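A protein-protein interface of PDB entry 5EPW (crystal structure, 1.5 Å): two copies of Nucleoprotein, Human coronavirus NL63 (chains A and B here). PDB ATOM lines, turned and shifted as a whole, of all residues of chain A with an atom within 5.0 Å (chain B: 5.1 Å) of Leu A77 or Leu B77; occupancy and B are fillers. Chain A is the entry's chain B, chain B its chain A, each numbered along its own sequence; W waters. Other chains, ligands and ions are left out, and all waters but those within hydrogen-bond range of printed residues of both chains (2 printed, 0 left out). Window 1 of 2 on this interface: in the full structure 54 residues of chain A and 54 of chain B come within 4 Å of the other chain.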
ATOM      1  N   ILE A  71      20.563  19.539  24.572  1.00  0.00           N
ATOM      2  CA  ILE A  71      21.047  20.804  25.215  1.00  0.00           C
ATOM      3  C   ILE A  71      21.147  21.798  24.082  1.00  0.00           C
ATOM      4  O   ILE A  71      21.847  21.565  23.063  1.00  0.00           O
ATOM      5  CB  ILE A  71      22.453  20.625  25.907  1.00  0.00           C
ATOM      6  CG1 ILE A  71      22.487  19.470  26.892  1.00  0.00           C
ATOM      7  CG2 ILE A  71      22.788  22.012  26.532  1.00  0.00           C
ATOM      8  CD1 ILE A  71      23.854  19.167  27.409  1.00  0.00           C
ATOM      9  N   PRO A  72      20.466  23.018  24.161  1.00  0.00           N
ATOM     10  CA  PRO A  72      20.711  23.982  23.082  1.00  0.00           C
ATOM     11  C   PRO A  72      22.096  24.497  22.920  1.00  0.00           C
ATOM     12  O   PRO A  72      22.845  24.605  23.971  1.00  0.00           O
ATOM     13  CB  PRO A  72      19.839  25.187  23.466  1.00  0.00           C
ATOM     14  CG  PRO A  72      19.709  24.994  24.888  1.00  0.00           C
ATOM     15  CD  PRO A  72      19.651  23.520  25.244  1.00  0.00           C
ATOM     16  N   ASN A  73      22.402  24.905  21.701  1.00  0.00           N
ATOM     17  CA  ASN A  73      23.632  25.576  21.456  1.00  0.00           C
ATOM     18  C   ASN A  73      23.640  27.019  21.866  1.00  0.00           C
ATOM     19  O   ASN A  73      22.596  27.553  22.304  1.00  0.00           O
ATOM     20  CB  ASN A  73      24.101  25.334  19.978  1.00  0.00           C
ATOM     21  CG  ASN A  73      23.320  26.162  18.998  1.00  0.00           C
ATOM     22  OD1 ASN A  73      23.317  27.476  19.103  1.00  0.00           O
ATOM     23  ND2 ASN A  73      22.619  25.483  18.093  1.00  0.00           N
ATOM     24  N   GLN A  74      24.780  27.693  21.860  1.00  0.00           N
ATOM     25  CA  GLN A  74      24.812  29.013  22.408  1.00  0.00           C
ATOM     26  C   GLN A  74      23.997  30.059  21.618  1.00  0.00           C
ATOM     27  O   GLN A  74      23.481  31.016  22.158  1.00  0.00           O
ATOM     28  CB  GLN A  74      26.274  29.496  22.425  1.00  0.00           C
ATOM     29  CG  GLN A  74      27.058  28.751  23.526  1.00  0.00           C
ATOM     30  CD  GLN A  74      28.454  29.079  23.578  1.00  0.00           C
ATOM     31  OE1 GLN A  74      28.818  30.253  23.568  1.00  0.00           O
ATOM     32  NE2 GLN A  74      29.309  28.051  23.643  1.00  0.00           N
ATOM     33  N   ALA A  75      23.910  29.870  20.306  1.00  0.00           N
ATOM     34  CA  ALA A  75      23.180  30.844  19.453  1.00  0.00           C
ATOM     35  C   ALA A  75      21.665  30.604  19.695  1.00  0.00           C
ATOM     36  O   ALA A  75      20.923  31.606  19.903  1.00  0.00           O
ATOM     37  CB  ALA A  75      23.544  30.613  17.992  1.00  0.00           C
ATOM     38  N   ALA A  76      21.208  29.380  19.804  1.00  0.00           N
ATOM     39  CA  ALA A  76      19.790  29.046  20.166  1.00  0.00           C
ATOM     40  C   ALA A  76      19.451  29.633  21.537  1.00  0.00           C
ATOM     41  O   ALA A  76      18.445  30.283  21.780  1.00  0.00           O
ATOM     42  CB  ALA A  76      19.431  27.577  20.140  1.00  0.00           C
ATOM     43  N   LEU A  77      20.359  29.472  22.526  1.00  0.00           N
ATOM     44  CA  LEU A  77      20.071  30.010  23.832  1.00  0.00           C
ATOM     45  C   LEU A  77      20.007  31.535  23.789  1.00  0.00           C
ATOM     46  O   LEU A  77      19.140  32.125  24.456  1.00  0.00           O
ATOM     47  CB  LEU A  77      21.197  29.587  24.857  1.00  0.00           C
ATOM     48  CG  LEU A  77      20.884  29.842  26.306  1.00  0.00           C
ATOM     49  CD1 LEU A  77      19.813  28.851  26.782  1.00  0.00           C
ATOM     50  CD2 LEU A  77      22.147  29.684  27.188  1.00  0.00           C
ATOM     51  N   PHE A  78      20.907  32.188  23.073  1.00  0.00           N
ATOM     52  CA  PHE A  78      20.856  33.656  22.993  1.00  0.00           C
ATOM     53  C   PHE A  78      19.559  34.163  22.356  1.00  0.00           C
ATOM     54  O   PHE A  78      18.914  35.063  22.886  1.00  0.00           O
ATOM     55  CB  PHE A  78      22.059  34.166  22.203  1.00  0.00           C
ATOM     56  CG  PHE A  78      22.230  35.672  22.207  1.00  0.00           C
ATOM     57  CD1 PHE A  78      22.803  36.328  23.249  1.00  0.00           C
ATOM     58  CD2 PHE A  78      21.765  36.345  21.148  1.00  0.00           C
ATOM     59  CE1 PHE A  78      22.922  37.730  23.230  1.00  0.00           C
ATOM     60  CE2 PHE A  78      21.899  37.721  21.061  1.00  0.00           C
ATOM     61  CZ  PHE A  78      22.472  38.403  22.080  1.00  0.00           C
ATOM     62  N   PHE A  79      19.253  33.650  21.200  1.00  0.00           N
ATOM     63  CA  PHE A  79      18.175  34.177  20.359  1.00  0.00           C
ATOM     64  C   PHE A  79      16.837  33.589  20.674  1.00  0.00           C
ATOM     65  O   PHE A  79      15.784  34.088  20.159  1.00  0.00           O
ATOM     66  CB  PHE A  79      18.459  33.974  18.873  1.00  0.00           C
ATOM     67  CG  PHE A  79      19.550  34.822  18.332  1.00  0.00           C
ATOM     68  CD1 PHE A  79      19.432  36.216  18.311  1.00  0.00           C
ATOM     69  CD2 PHE A  79      20.780  34.248  17.914  1.00  0.00           C
ATOM     70  CE1 PHE A  79      20.433  37.027  17.833  1.00  0.00           C
ATOM     71  CE2 PHE A  79      21.779  35.056  17.372  1.00  0.00           C
ATOM     72  CZ  PHE A  79      21.580  36.421  17.300  1.00  0.00           C
ATOM     73  N   ASP A  80      16.727  32.531  21.470  1.00  0.00           N
ATOM     74  CA  ASP A  80      15.472  31.805  21.620  1.00  0.00           C
ATOM     75  C   ASP A  80      15.123  31.569  23.094  1.00  0.00           C
ATOM     76  O   ASP A  80      14.301  30.717  23.407  1.00  0.00           O
ATOM     77  CB  ASP A  80      15.447  30.525  20.772  1.00  0.00           C
ATOM     78  CG  ASP A  80      14.051  29.974  20.516  1.00  0.00           C
ATOM     79  OD1 ASP A  80      13.165  30.857  20.283  1.00  0.00           O
ATOM     80  OD2 ASP A  80      13.939  28.746  20.376  1.00  0.00           O
ATOM     81  N   SER A  81      15.646  32.433  23.975  1.00  0.00           N
ATOM     82  CA  SER A  81      15.332  32.490  25.430  1.00  0.00           C
ATOM     83  C   SER A  81      14.665  33.810  25.792  1.00  0.00           C
ATOM     84  O   SER A  81      14.804  34.844  25.109  1.00  0.00           O
ATOM     85  CB  SER A  81      16.626  32.396  26.294  1.00  0.00           C
ATOM     86  OG  SER A  81      17.351  31.167  26.098  1.00  0.00           O
ATOM     87  N   TYR A  96      18.740  33.299  31.999  1.00  0.00           N
ATOM     88  CA  TYR A  96      18.189  32.742  30.774  1.00  0.00           C
ATOM     89  C   TYR A  96      17.090  31.761  31.159  1.00  0.00           C
ATOM     90  O   TYR A  96      17.365  30.818  31.917  1.00  0.00           O
ATOM     91  CB  TYR A  96      19.230  32.012  29.934  1.00  0.00           C
ATOM     92  CG  TYR A  96      20.368  32.817  29.355  1.00  0.00           C
ATOM     93  CD1 TYR A  96      21.473  33.174  30.138  1.00  0.00           C
ATOM     94  CD2 TYR A  96      20.371  33.074  27.958  1.00  0.00           C
ATOM     95  CE1 TYR A  96      22.557  33.801  29.529  1.00  0.00           C
ATOM     96  CE2 TYR A  96      21.477  33.692  27.342  1.00  0.00           C
ATOM     97  CZ  TYR A  96      22.496  34.075  28.158  1.00  0.00           C
ATOM     98  OH  TYR A  96      23.612  34.685  27.555  1.00  0.00           O
ATOM     99  N   TYR A  98      14.867  29.163  29.094  1.00  0.00           N
ATOM    100  CA  TYR A  98      14.830  28.570  27.735  1.00  0.00           C
ATOM    101  C   TYR A  98      13.819  27.392  27.777  1.00  0.00           C
ATOM    102  O   TYR A  98      14.010  26.487  28.581  1.00  0.00           O
ATOM    103  CB  TYR A  98      16.246  28.126  27.307  1.00  0.00           C
ATOM    104  CG  TYR A  98      16.222  27.479  25.935  1.00  0.00           C
ATOM    105  CD1 TYR A  98      16.160  28.262  24.809  1.00  0.00           C
ATOM    106  CD2 TYR A  98      16.094  26.096  25.815  1.00  0.00           C
ATOM    107  CE1 TYR A  98      16.019  27.649  23.506  1.00  0.00           C
ATOM    108  CE2 TYR A  98      16.009  25.512  24.577  1.00  0.00           C
ATOM    109  CZ  TYR A  98      15.981  26.272  23.451  1.00  0.00           C
ATOM    110  OH  TYR A  98      15.870  25.631  22.229  1.00  0.00           O
ATOM    111  N   ILE B  71      27.497  33.899  27.100  1.00  0.00           N
ATOM    112  CA  ILE B  71      26.504  32.802  26.876  1.00  0.00           C
ATOM    113  C   ILE B  71      27.133  31.519  27.467  1.00  0.00           C
ATOM    114  O   ILE B  71      28.266  31.159  27.167  1.00  0.00           O
ATOM    115  CB  ILE B  71      26.174  32.581  25.465  1.00  0.00           C
ATOM    116  CG1 ILE B  71      25.758  33.840  24.692  1.00  0.00           C
ATOM    117  CG2 ILE B  71      25.026  31.561  25.364  1.00  0.00           C
ATOM    118  CD1 ILE B  71      25.617  33.627  23.235  1.00  0.00           C
ATOM    119  N   PRO B  72      26.389  30.797  28.373  1.00  0.00           N
ATOM    120  CA  PRO B  72      26.969  29.520  28.915  1.00  0.00           C
ATOM    121  C   PRO B  72      27.163  28.486  27.812  1.00  0.00           C
ATOM    122  O   PRO B  72      26.375  28.390  26.850  1.00  0.00           O
ATOM    123  CB  PRO B  72      25.916  29.035  29.925  1.00  0.00           C
ATOM    124  CG  PRO B  72      24.686  29.642  29.396  1.00  0.00           C
ATOM    125  CD  PRO B  72      25.061  31.081  28.929  1.00  0.00           C
ATOM    126  N   ASN B  73      28.195  27.644  27.949  1.00  0.00           N
ATOM    127  CA  ASN B  73      28.385  26.495  27.141  1.00  0.00           C
ATOM    128  C   ASN B  73      27.463  25.341  27.491  1.00  0.00           C
ATOM    129  O   ASN B  73      26.623  25.507  28.399  1.00  0.00           O
ATOM    130  CB  ASN B  73      29.872  26.106  27.152  1.00  0.00           C
ATOM    131  CG  ASN B  73      30.312  25.496  28.427  1.00  0.00           C
ATOM    132  OD1 ASN B  73      29.491  24.917  29.122  1.00  0.00           O
ATOM    133  ND2 ASN B  73      31.527  25.670  28.809  1.00  0.00           N
ATOM    134  N   GLN B  74      27.453  24.253  26.676  1.00  0.00           N
ATOM    135  CA  GLN B  74      26.447  23.227  26.896  1.00  0.00           C
ATOM    136  C   GLN B  74      26.610  22.545  28.252  1.00  0.00           C
ATOM    137  O   GLN B  74      25.614  22.218  28.903  1.00  0.00           O
ATOM    138  CB  GLN B  74      26.333  22.162  25.736  1.00  0.00           C
ATOM    139  CG  GLN B  74      25.751  22.759  24.418  1.00  0.00           C
ATOM    140  CD  GLN B  74      25.325  21.759  23.278  1.00  0.00           C
ATOM    141  OE1 GLN B  74      25.640  20.580  23.234  1.00  0.00           O
ATOM    142  NE2 GLN B  74      24.510  22.238  22.468  1.00  0.00           N
ATOM    143  N   ALA B  75      27.836  22.318  28.687  1.00  0.00           N
ATOM    144  CA  ALA B  75      28.094  21.700  29.982  1.00  0.00           C
ATOM    145  C   ALA B  75      27.628  22.500  31.185  1.00  0.00           C
ATOM    146  O   ALA B  75      26.943  22.046  32.099  1.00  0.00           O
ATOM    147  CB  ALA B  75      29.579  21.374  30.169  1.00  0.00           C
ATOM    148  N   ALA B  76      27.909  23.815  31.109  1.00  0.00           N
ATOM    149  CA  ALA B  76      27.444  24.732  32.124  1.00  0.00           C
ATOM    150  C   ALA B  76      25.917  24.824  32.124  1.00  0.00           C
ATOM    151  O   ALA B  76      25.275  24.831  33.186  1.00  0.00           O
ATOM    152  CB  ALA B  76      28.107  26.174  31.881  1.00  0.00           C
ATOM    153  N   LEU B  77      25.284  24.952  30.963  1.00  0.00           N
ATOM    154  CA  LEU B  77      23.835  24.967  30.909  1.00  0.00           C
ATOM    155  C   LEU B  77      23.308  23.715  31.550  1.00  0.00           C
ATOM    156  O   LEU B  77      22.297  23.717  32.323  1.00  0.00           O
ATOM    157  CB  LEU B  77      23.285  25.101  29.450  1.00  0.00           C
ATOM    158  CG  LEU B  77      21.793  25.400  29.383  1.00  0.00           C
ATOM    159  CD1 LEU B  77      21.519  26.797  29.874  1.00  0.00           C
ATOM    160  CD2 LEU B  77      21.403  25.286  27.964  1.00  0.00           C
ATOM    161  N   PHE B  78      23.845  22.543  31.228  1.00  0.00           N
ATOM    162  CA  PHE B  78      23.309  21.312  31.760  1.00  0.00           C
ATOM    163  C   PHE B  78      23.446  21.153  33.248  1.00  0.00           C
ATOM    164  O   PHE B  78      22.535  20.771  33.995  1.00  0.00           O
ATOM    165  CB  PHE B  78      24.000  20.105  31.041  1.00  0.00           C
ATOM    166  CG  PHE B  78      23.453  18.730  31.415  1.00  0.00           C
ATOM    167  CD1 PHE B  78      22.330  18.249  30.830  1.00  0.00           C
ATOM    168  CD2 PHE B  78      24.123  17.959  32.305  1.00  0.00           C
ATOM    169  CE1 PHE B  78      21.858  16.978  31.175  1.00  0.00           C
ATOM    170  CE2 PHE B  78      23.650  16.682  32.657  1.00  0.00           C
ATOM    171  CZ  PHE B  78      22.502  16.234  32.055  1.00  0.00           C
ATOM    172  N   PHE B  79      24.676  21.419  33.746  1.00  0.00           N
ATOM    173  CA  PHE B  79      25.057  21.140  35.142  1.00  0.00           C
ATOM    174  C   PHE B  79      24.747  22.324  36.059  1.00  0.00           C
ATOM    175  O   PHE B  79      24.796  22.147  37.266  1.00  0.00           O
ATOM    176  CB  PHE B  79      26.529  20.752  35.230  1.00  0.00           C
ATOM    177  CG  PHE B  79      26.856  19.401  34.671  1.00  0.00           C
ATOM    178  CD1 PHE B  79      26.306  18.221  35.308  1.00  0.00           C
ATOM    179  CD2 PHE B  79      27.652  19.211  33.600  1.00  0.00           C
ATOM    180  CE1 PHE B  79      26.628  17.016  34.816  1.00  0.00           C
ATOM    181  CE2 PHE B  79      28.012  17.961  33.143  1.00  0.00           C
ATOM    182  CZ  PHE B  79      27.474  16.827  33.793  1.00  0.00           C
ATOM    183  N   ASP B  80      24.471  23.521  35.564  1.00  0.00           N
ATOM    184  CA  ASP B  80      24.306  24.647  36.403  1.00  0.00           C
ATOM    185  C   ASP B  80      22.998  25.326  36.266  1.00  0.00           C
ATOM    186  O   ASP B  80      22.794  26.480  36.730  1.00  0.00           O
ATOM    187  CB  ASP B  80      25.508  25.643  36.159  1.00  0.00           C
ATOM    188  CG  ASP B  80      26.012  26.279  37.405  1.00  0.00           C
ATOM    189  OD1 ASP B  80      25.794  25.800  38.521  1.00  0.00           O
ATOM    190  OD2 ASP B  80      26.724  27.328  37.188  1.00  0.00           O
ATOM    191  N   SER B  81      22.007  24.654  35.669  1.00  0.00           N
ATOM    192  CA  SER B  81      20.637  25.058  35.529  1.00  0.00           C
ATOM    193  C   SER B  81      19.688  24.342  36.506  1.00  0.00           C
ATOM    194  O   SER B  81      19.995  23.249  36.955  1.00  0.00           O
ATOM    195  CB  SER B  81      20.065  24.836  34.185  1.00  0.00           C
ATOM    196  OG  SER B  81      20.685  25.631  33.147  1.00  0.00           O
ATOM    197  N   TYR B  96      14.922  25.080  30.890  1.00  0.00           N
ATOM    198  CA  TYR B  96      16.162  25.342  31.538  1.00  0.00           C
ATOM    199  C   TYR B  96      16.092  26.781  32.134  1.00  0.00           C
ATOM    200  O   TYR B  96      15.871  27.765  31.428  1.00  0.00           O
ATOM    201  CB  TYR B  96      17.395  25.363  30.592  1.00  0.00           C
ATOM    202  CG  TYR B  96      17.794  24.041  29.963  1.00  0.00           C
ATOM    203  CD1 TYR B  96      17.114  23.514  28.836  1.00  0.00           C
ATOM    204  CD2 TYR B  96      18.910  23.340  30.446  1.00  0.00           C
ATOM    205  CE1 TYR B  96      17.540  22.321  28.291  1.00  0.00           C
ATOM    206  CE2 TYR B  96      19.313  22.179  29.841  1.00  0.00           C
ATOM    207  CZ  TYR B  96      18.624  21.697  28.779  1.00  0.00           C
ATOM    208  OH  TYR B  96      19.230  20.528  28.254  1.00  0.00           O
ATOM    209  N   TYR B  98      18.605  29.265  33.914  1.00  0.00           N
ATOM    210  CA  TYR B  98      20.035  29.376  34.148  1.00  0.00           C
ATOM    211  C   TYR B  98      20.395  30.765  34.632  1.00  0.00           C
ATOM    212  O   TYR B  98      19.998  31.748  33.995  1.00  0.00           O
ATOM    213  CB  TYR B  98      20.819  29.061  32.834  1.00  0.00           C
ATOM    214  CG  TYR B  98      22.276  29.203  32.948  1.00  0.00           C
ATOM    215  CD1 TYR B  98      23.041  28.183  33.434  1.00  0.00           C
ATOM    216  CD2 TYR B  98      22.926  30.423  32.640  1.00  0.00           C
ATOM    217  CE1 TYR B  98      24.402  28.311  33.616  1.00  0.00           C
ATOM    218  CE2 TYR B  98      24.210  30.543  32.902  1.00  0.00           C
ATOM    219  CZ  TYR B  98      24.951  29.539  33.383  1.00  0.00           C
ATOM    220  OH  TYR B  98      26.312  29.689  33.636  1.00  0.00           O
HETATM  221  O   HOH W   1      28.754  24.898  24.022  1.00  0.00           O
HETATM  222  O   HOH W   2      25.181  26.206  24.975  1.00  0.00           O
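Water W2 lies within hydrogen-bond range of O of Pro A72 (3.0 Å), O of Pro B72 (3.1 Å), N of Gln B74 (3.4 Å) and N of Gln A74 (3.5 Å).
Water W1 bridges the backbone NH (N) of Gln B74 (3.0 Å) and the side-chain amide nitrogen (NE2) of Gln A74 (3.2 Å).
Printed residues of chain A that touch a printed residue of chain B: Ile A71, Pro A72, Asn A73, Gln A74, Leu A77, Phe A78, Tyr A96 and Tyr A98.
Hydrophobic or aromatic side chains of chain A that line the printed part of chain B: Ile A71, Pro A72, Leu A77, Phe A78 and Tyr A96.
Among the printed residues, 20 pairs touch across the chains.
Among the printed residues, no Asp or Glu carboxylate lies within 4 Å of a Lys or Arg side-chain nitrogen of the other chain.
Ile A71 touches Gln B74, and with the chains exchanged Gln A74 touches Ile B71.
Pro A72 touches Leu B77, and with the chains exchanged Leu A77 touches Pro B72.
Tyr A96 touches its own counterpart, Tyr B96.
Tyr A96 touches Tyr B98, and with the chains exchanged Tyr A98 touches Tyr B96.
Positions printed for both chains: 71, 72, 73, 74, 75, 76, 77, 78, 79, 80, 81, 96 and 98.
Of the 20 pairs that touch across the chains among the printed residues, 20 have their exchanged pair printed and touching as well.
O of Ile A71 sits at hydrogen-bond distance from NE2 of Gln B74.
The backbone carbonyl oxygen (O) of Pro A72 lies within hydrogen-bond range of the side-chain amide nitrogen (NE2) of Gln B74 (3.3 Å).
NE2 of Gln B74 sits close to N of Asn A73, 3.5 Å away.
O of Tyr A98 is in hydrogen-bond range of N of Tyr B96, at 2.9 Å.
The backbone NH of Tyr B98 lies within hydrogen-bond range of the backbone carbonyl oxygen of Tyr A96 (2.8 Å).
O of Tyr B96 lies close to O of Tyr A96 (3.4 Å).
N of Ala B75 lies within hydrogen-bond range of OD1 of Asn B73 (3.1 Å).
The backbone NH (N) of Ala B76 is in hydrogen-bond range of the side-chain amide oxygen (OD1) of Asn B73, at 2.8 Å.
O of Leu B77 is in hydrogen-bond range of OG of Ser B81, at 2.6 Å.
The side-chain amide oxygen (OD1) of Asn A73 is in hydrogen-bond range of the backbone NH (N) of Ala A75.
The backbone NH (N) of Ala A76 lies within hydrogen-bond range of the side-chain amide oxygen (OD1) of Asn A73, 2.9 Å away.
O of Leu A77 is in hydrogen-bond range of OG of Ser A81 (2.6 Å).
Of the printed residues of chain B, Leu A77 touches Ile B71, Pro B72 and Leu B77.
Printed residues of chain B within 4 Å of Tyr A96: Ile B71 (3.5 Å), Pro B72 (3.7 Å), Tyr B96 (3.4 Å) and Tyr B98 (2.8 Å).
Of the printed residues of chain A, Pro B72 touches Gln A74 (3.4 Å), Leu A77 (3.4 Å) and Tyr A96 (3.7 Å).
Printed residues of chain A within 4 Å of Asn B73: Gln A74 (3.9 Å).
Of the printed residues of chain A, Leu B77 touches Ile A71 (3.8 Å), Pro A72 (3.5 Å) and Leu A77 (3.99 Å).
The nearest printed residue of chain B that does not touch Leu A77 is Tyr B98 (5.6 Å).
The nearest printed residue of chain A that does not touch Ile B71 is Ala A75 (5.1 Å).
Leu B77 touches Ile A71.
Ile A71 touches Tyr B96 (CA to OH, 3.6 Å).
CG of Pro A72 touches CD2 of Leu B77, at 3.5 Å.
Pro A72 touches Tyr B96.
Gln A74 touches Ile B71.
Gln A74 touches Pro B72.
Gln A74 touches Asn B73.
Ile B71 touches Leu A77 (CG2 to CD2, 3.9 Å).
Phe A78 touches Ile B71.
CE1 of Tyr A96 touches CD of Pro B72, 3.7 Å away.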
